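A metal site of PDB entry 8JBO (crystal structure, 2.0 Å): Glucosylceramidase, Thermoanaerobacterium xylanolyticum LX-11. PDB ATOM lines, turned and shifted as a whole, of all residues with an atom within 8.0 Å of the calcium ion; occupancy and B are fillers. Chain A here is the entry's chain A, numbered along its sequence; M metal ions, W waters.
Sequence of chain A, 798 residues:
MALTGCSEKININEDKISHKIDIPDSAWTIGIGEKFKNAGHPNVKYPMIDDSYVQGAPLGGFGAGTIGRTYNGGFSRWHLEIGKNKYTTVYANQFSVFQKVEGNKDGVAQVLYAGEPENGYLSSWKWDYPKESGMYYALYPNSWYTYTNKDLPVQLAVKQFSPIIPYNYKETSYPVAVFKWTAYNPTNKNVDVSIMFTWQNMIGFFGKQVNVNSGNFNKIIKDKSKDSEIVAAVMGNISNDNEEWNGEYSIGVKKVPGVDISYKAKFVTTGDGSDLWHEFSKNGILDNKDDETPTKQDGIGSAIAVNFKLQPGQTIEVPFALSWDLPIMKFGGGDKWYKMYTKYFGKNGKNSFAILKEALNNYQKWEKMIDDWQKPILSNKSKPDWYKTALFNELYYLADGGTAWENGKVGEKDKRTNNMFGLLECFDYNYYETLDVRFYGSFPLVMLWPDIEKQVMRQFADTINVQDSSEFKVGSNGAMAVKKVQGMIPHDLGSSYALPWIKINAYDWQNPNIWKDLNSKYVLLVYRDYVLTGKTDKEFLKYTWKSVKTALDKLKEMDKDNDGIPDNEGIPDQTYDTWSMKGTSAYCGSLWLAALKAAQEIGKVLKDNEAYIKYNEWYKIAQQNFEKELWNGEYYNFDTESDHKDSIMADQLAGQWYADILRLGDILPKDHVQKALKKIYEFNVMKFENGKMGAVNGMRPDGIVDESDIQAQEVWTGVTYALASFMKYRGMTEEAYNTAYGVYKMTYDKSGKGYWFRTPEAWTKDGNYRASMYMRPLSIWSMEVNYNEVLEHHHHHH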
ATOM      1  N   LYS A 556     -13.613 -16.783  11.113  1.00  0.00           N
ATOM      2  CA  LYS A 556     -14.735 -15.838  11.033  1.00  0.00           C
ATOM      3  C   LYS A 556     -14.517 -14.615  11.937  1.00  0.00           C
ATOM      4  O   LYS A 556     -14.908 -13.505  11.574  1.00  0.00           O
ATOM      5  CB  LYS A 556     -16.057 -16.539  11.399  1.00  0.00           C
ATOM      6  CG  LYS A 556     -17.311 -15.676  11.369  1.00  0.00           C
ATOM      7  CD  LYS A 556     -17.499 -15.030   9.998  1.00  0.00           C
ATOM      8  CE  LYS A 556     -18.942 -14.878   9.620  1.00  0.00           C
ATOM      9  NZ  LYS A 556     -19.608 -13.915  10.506  1.00  0.00           N
ATOM     10  N   MET A 558     -11.826 -13.101  12.367  1.00  0.00           N
ATOM     11  CA  MET A 558     -10.906 -12.173  11.697  1.00  0.00           C
ATOM     12  C   MET A 558     -11.568 -11.282  10.649  1.00  0.00           C
ATOM     13  O   MET A 558     -10.884 -10.481  10.006  1.00  0.00           O
ATOM     14  CB  MET A 558      -9.711 -12.930  11.072  1.00  0.00           C
ATOM     15  CG  MET A 558      -8.787 -13.534  12.094  1.00  0.00           C
ATOM     16  SD  MET A 558      -7.753 -14.847  11.395  1.00  0.00           S
ATOM     17  CE  MET A 558      -6.846 -15.282  12.877  1.00  0.00           C
ATOM     18  N   ASP A 559     -12.875 -11.425  10.470  1.00  0.00           N
ATOM     19  CA  ASP A 559     -13.669 -10.475   9.674  1.00  0.00           C
ATOM     20  C   ASP A 559     -13.817  -9.186  10.496  1.00  0.00           C
ATOM     21  O   ASP A 559     -14.542  -9.174  11.473  1.00  0.00           O
ATOM     22  CB  ASP A 559     -15.046 -11.089   9.342  1.00  0.00           C
ATOM     23  CG  ASP A 559     -15.954 -10.114   8.572  1.00  0.00           C
ATOM     24  OD1 ASP A 559     -15.452  -9.145   8.010  1.00  0.00           O
ATOM     25  OD2 ASP A 559     -17.176 -10.348   8.519  1.00  0.00           O
ATOM     26  N   LYS A 560     -13.099  -8.130  10.108  1.00  0.00           N
ATOM     27  CA  LYS A 560     -13.101  -6.822  10.805  1.00  0.00           C
ATOM     28  C   LYS A 560     -14.327  -5.971  10.503  1.00  0.00           C
ATOM     29  O   LYS A 560     -14.874  -5.329  11.383  1.00  0.00           O
ATOM     30  CB  LYS A 560     -11.863  -5.981  10.447  1.00  0.00           C
ATOM     31  CG  LYS A 560     -10.491  -6.504  10.866  1.00  0.00           C
ATOM     32  CD  LYS A 560     -10.404  -6.744  12.369  1.00  0.00           C
ATOM     33  CE  LYS A 560     -10.797  -8.168  12.758  1.00  0.00           C
ATOM     34  NZ  LYS A 560     -11.624  -8.224  13.998  1.00  0.00           N
ATOM     35  N   ASP A 561     -14.729  -5.938   9.239  1.00  0.00           N
ATOM     36  CA  ASP A 561     -15.710  -4.973   8.749  1.00  0.00           C
ATOM     37  C   ASP A 561     -17.082  -5.586   8.501  1.00  0.00           C
ATOM     38  O   ASP A 561     -17.930  -4.995   7.856  1.00  0.00           O
ATOM     39  CB  ASP A 561     -15.168  -4.293   7.486  1.00  0.00           C
ATOM     40  CG  ASP A 561     -14.889  -5.262   6.341  1.00  0.00           C
ATOM     41  OD1 ASP A 561     -15.208  -6.475   6.413  1.00  0.00           O
ATOM     42  OD2 ASP A 561     -14.314  -4.808   5.337  1.00  0.00           O
ATOM     43  N   ASN A 562     -17.307  -6.800   8.997  1.00  0.00           N
ATOM     44  CA  ASN A 562     -18.601  -7.436   8.903  1.00  0.00           C
ATOM     45  C   ASN A 562     -19.141  -7.678   7.474  1.00  0.00           C
ATOM     46  O   ASN A 562     -20.361  -7.738   7.270  1.00  0.00           O
ATOM     47  CB  ASN A 562     -19.635  -6.677   9.760  1.00  0.00           C
ATOM     48  CG  ASN A 562     -20.697  -7.613  10.330  1.00  0.00           C
ATOM     49  OD1 ASN A 562     -20.371  -8.596  11.002  1.00  0.00           O
ATOM     50  ND2 ASN A 562     -21.964  -7.337  10.043  1.00  0.00           N
ATOM     51  N   ASP A 563     -18.248  -7.876   6.485  1.00  0.00           N
ATOM     52  CA  ASP A 563     -18.678  -8.358   5.164  1.00  0.00           C
ATOM     53  C   ASP A 563     -18.788  -9.884   5.041  1.00  0.00           C
ATOM     54  O   ASP A 563     -19.058 -10.406   3.944  1.00  0.00           O
ATOM     55  CB  ASP A 563     -17.828  -7.779   4.026  1.00  0.00           C
ATOM     56  CG  ASP A 563     -16.408  -8.393   3.927  1.00  0.00           C
ATOM     57  OD1 ASP A 563     -15.881  -9.045   4.887  1.00  0.00           O
ATOM     58  OD2 ASP A 563     -15.795  -8.137   2.883  1.00  0.00           O
ATOM     59  N   GLY A 564     -18.596 -10.586   6.161  1.00  0.00           N
ATOM     60  CA  GLY A 564     -18.710 -12.032   6.235  1.00  0.00           C
ATOM     61  C   GLY A 564     -17.462 -12.788   5.771  1.00  0.00           C
ATOM     62  O   GLY A 564     -17.481 -14.023   5.721  1.00  0.00           O
ATOM     63  N   ILE A 565     -16.385 -12.051   5.486  1.00  0.00           N
ATOM     64  CA  ILE A 565     -15.156 -12.610   4.928  1.00  0.00           C
ATOM     65  C   ILE A 565     -13.986 -12.181   5.811  1.00  0.00           C
ATOM     66  O   ILE A 565     -13.914 -11.015   6.175  1.00  0.00           O
ATOM     67  CB  ILE A 565     -14.921 -12.115   3.477  1.00  0.00           C
ATOM     68  CG1 ILE A 565     -16.119 -12.437   2.596  1.00  0.00           C
ATOM     69  CG2 ILE A 565     -13.638 -12.720   2.883  1.00  0.00           C
ATOM     70  CD1 ILE A 565     -16.083 -11.704   1.258  1.00  0.00           C
ATOM     71  N   PRO A 566     -13.032 -13.094   6.115  1.00  0.00           N
ATOM     72  CA  PRO A 566     -11.834 -12.660   6.850  1.00  0.00           C
ATOM     73  C   PRO A 566     -11.067 -11.558   6.114  1.00  0.00           C
ATOM     74  O   PRO A 566     -11.019 -11.560   4.901  1.00  0.00           O
ATOM     75  CB  PRO A 566     -10.968 -13.917   6.924  1.00  0.00           C
ATOM     76  CG  PRO A 566     -11.887 -15.048   6.645  1.00  0.00           C
ATOM     77  CD  PRO A 566     -13.031 -14.538   5.842  1.00  0.00           C
ATOM     78  N   ASP A 567     -10.482 -10.638   6.873  1.00  0.00           N
ATOM     79  CA  ASP A 567      -9.752  -9.493   6.326  1.00  0.00           C
ATOM     80  C   ASP A 567      -8.266  -9.809   6.320  1.00  0.00           C
ATOM     81  O   ASP A 567      -7.706 -10.010   7.394  1.00  0.00           O
ATOM     82  CB  ASP A 567      -9.957  -8.247   7.203  1.00  0.00           C
ATOM     83  CG  ASP A 567     -11.297  -7.589   6.985  1.00  0.00           C
ATOM     84  OD1 ASP A 567     -12.347  -8.209   7.337  1.00  0.00           O
ATOM     85  OD2 ASP A 567     -11.271  -6.445   6.456  1.00  0.00           O
ATOM     86  N   ASN A 568      -7.634  -9.809   5.151  1.00  0.00           N
ATOM     87  CA  ASN A 568      -6.156  -9.783   5.079  1.00  0.00           C
ATOM     88  C   ASN A 568      -5.675  -8.463   5.695  1.00  0.00           C
ATOM     89  O   ASN A 568      -6.309  -7.434   5.537  1.00  0.00           O
ATOM     90  CB  ASN A 568      -5.637  -9.985   3.636  1.00  0.00           C
ATOM     91  CG  ASN A 568      -5.990 -11.384   3.067  1.00  0.00           C
ATOM     92  OD1 ASN A 568      -6.985 -11.534   2.358  1.00  0.00           O
ATOM     93  ND2 ASN A 568      -5.189 -12.399   3.399  1.00  0.00           N
ATOM     94  N   GLY A 583      -7.679  -6.440   3.028  1.00  0.00           N
ATOM     95  CA  GLY A 583      -9.094  -6.422   2.831  1.00  0.00           C
ATOM     96  C   GLY A 583      -9.569  -7.801   2.472  1.00  0.00           C
ATOM     97  O   GLY A 583      -9.102  -8.796   3.023  1.00  0.00           O
ATOM     98  N   THR A 584     -10.539  -7.858   1.578  1.00  0.00           N
ATOM     99  CA  THR A 584     -10.936  -9.110   0.971  1.00  0.00           C
ATOM    100  C   THR A 584      -9.988  -9.374  -0.201  1.00  0.00           C
ATOM    101  O   THR A 584      -9.866  -8.524  -1.090  1.00  0.00           O
ATOM    102  CB  THR A 584     -12.364  -9.031   0.456  1.00  0.00           C
ATOM    103  OG1 THR A 584     -13.250  -8.819   1.558  1.00  0.00           O
ATOM    104  CG2 THR A 584     -12.790 -10.345  -0.264  1.00  0.00           C
ATOM    105  N   TRP A 592     -12.014 -19.307   1.489  1.00  0.00           N
ATOM    106  CA  TRP A 592     -13.033 -19.212   2.528  1.00  0.00           C
ATOM    107  C   TRP A 592     -14.418 -19.668   2.061  1.00  0.00           C
ATOM    108  O   TRP A 592     -15.076 -20.458   2.747  1.00  0.00           O
ATOM    109  CB  TRP A 592     -13.069 -17.753   3.014  1.00  0.00           C
ATOM    110  CG  TRP A 592     -14.172 -17.369   3.954  1.00  0.00           C
ATOM    111  CD1 TRP A 592     -15.145 -16.433   3.708  1.00  0.00           C
ATOM    112  CD2 TRP A 592     -14.383 -17.833   5.290  1.00  0.00           C
ATOM    113  NE1 TRP A 592     -15.966 -16.306   4.804  1.00  0.00           N
ATOM    114  CE2 TRP A 592     -15.526 -17.153   5.798  1.00  0.00           C
ATOM    115  CE3 TRP A 592     -13.726 -18.755   6.110  1.00  0.00           C
ATOM    116  CZ2 TRP A 592     -16.016 -17.366   7.093  1.00  0.00           C
ATOM    117  CZ3 TRP A 592     -14.229 -18.985   7.411  1.00  0.00           C
ATOM    118  CH2 TRP A 592     -15.367 -18.280   7.883  1.00  0.00           C
ATOM    119  N   ASN A 625     -20.989 -10.832  -1.054  1.00  0.00           N
ATOM    120  CA  ASN A 625     -20.040  -9.742  -0.887  1.00  0.00           C
ATOM    121  C   ASN A 625     -18.726  -9.925  -1.650  1.00  0.00           C
ATOM    122  O   ASN A 625     -18.142  -8.959  -2.123  1.00  0.00           O
ATOM    123  CB  ASN A 625     -19.773  -9.453   0.599  1.00  0.00           C
ATOM    124  CG  ASN A 625     -21.002  -8.882   1.314  1.00  0.00           C
ATOM    125  OD1 ASN A 625     -21.857  -8.307   0.694  1.00  0.00           O
ATOM    126  ND2 ASN A 625     -21.078  -9.079   2.615  1.00  0.00           N
ATOM    127  N   GLU A 629     -17.501  -7.162  -4.235  1.00  0.00           N
ATOM    128  CA  GLU A 629     -16.227  -6.483  -3.936  1.00  0.00           C
ATOM    129  C   GLU A 629     -15.139  -6.675  -4.992  1.00  0.00           C
ATOM    130  O   GLU A 629     -14.286  -5.800  -5.169  1.00  0.00           O
ATOM    131  CB  GLU A 629     -15.681  -6.919  -2.575  1.00  0.00           C
ATOM    132  CG  GLU A 629     -16.471  -6.405  -1.391  1.00  0.00           C
ATOM    133  CD  GLU A 629     -16.077  -7.061  -0.110  1.00  0.00           C
ATOM    134  OE1 GLU A 629     -14.958  -7.632  -0.004  1.00  0.00           O
ATOM    135  OE2 GLU A 629     -16.890  -7.007   0.831  1.00  0.00           O
ATOM    136  N   THR A 640      -9.191  -5.814  -2.117  1.00  0.00           N
ATOM    137  CA  THR A 640      -9.970  -4.559  -2.020  1.00  0.00           C
ATOM    138  C   THR A 640      -9.201  -3.323  -1.549  1.00  0.00           C
ATOM    139  O   THR A 640      -9.689  -2.223  -1.740  1.00  0.00           O
ATOM    140  CB  THR A 640     -11.177  -4.730  -1.076  1.00  0.00           C
ATOM    141  OG1 THR A 640     -10.741  -5.244   0.169  1.00  0.00           O
ATOM    142  CG2 THR A 640     -12.177  -5.652  -1.651  1.00  0.00           C
ATOM    143  N   GLU A 641      -8.022  -3.478  -0.954  1.00  0.00           N
ATOM    144  CA  GLU A 641      -7.342  -2.361  -0.274  1.00  0.00           C
ATOM    145  C   GLU A 641      -5.841  -2.150  -0.537  1.00  0.00           C
ATOM    146  O   GLU A 641      -5.265  -1.243   0.035  1.00  0.00           O
ATOM    147  CB  GLU A 641      -7.569  -2.489   1.243  1.00  0.00           C
ATOM    148  CG  GLU A 641      -8.996  -2.225   1.699  1.00  0.00           C
ATOM    149  CD  GLU A 641      -9.223  -2.534   3.176  1.00  0.00           C
ATOM    150  OE1 GLU A 641      -8.352  -2.210   4.010  1.00  0.00           O
ATOM    151  OE2 GLU A 641     -10.266  -3.119   3.491  1.00  0.00           O
HETATM  152 CA    CA M   1     -14.141  -8.691   6.057  1.00  0.00          CA
HETATM  153  O   HOH W   1     -12.461  -9.036   4.313  1.00  0.00           O
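OG1 of Thr 584 sits at hydrogen-bond distance from OD2 of Asp 563.
The side-chain carboxylate (OD2) of Asp 563 lies close to the side-chain carboxylate (OE2) of Glu 629 (2.6 Å).
ND2 of Asn 625 lies within hydrogen-bond range of O of Asp 563, at 2.8 Å.
OD1 of Asp 567 lies close to N of Lys 560 (2.9 Å).
The backbone carbonyl oxygen of Met 558 sits at hydrogen-bond distance from the backbone NH of Asp 567 (3.2 Å).
OD1 of Asp 559 lies close to N of Asn 562 (3.1 Å).
The side-chain carboxylate (OD2) of Asp 559 lies within hydrogen-bond range of the backbone NH (N) of Gly 564, 2.8 Å away.
The calcium ion is bound by OD1 of Asp 563, OD1 of Asp 567, O of Ile 565, OD1 of Asp 559, water W1 and OD1 of Asp 561.
Of the 19 residues printed, 5 come within 4 Å of the calcium ion.
Water W1 lies within hydrogen-bond range of the side-chain hydroxyl (OG1) of Thr 584 (2.9 Å) and the backbone carbonyl oxygen (O) of Pro 566 (3.0 Å).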
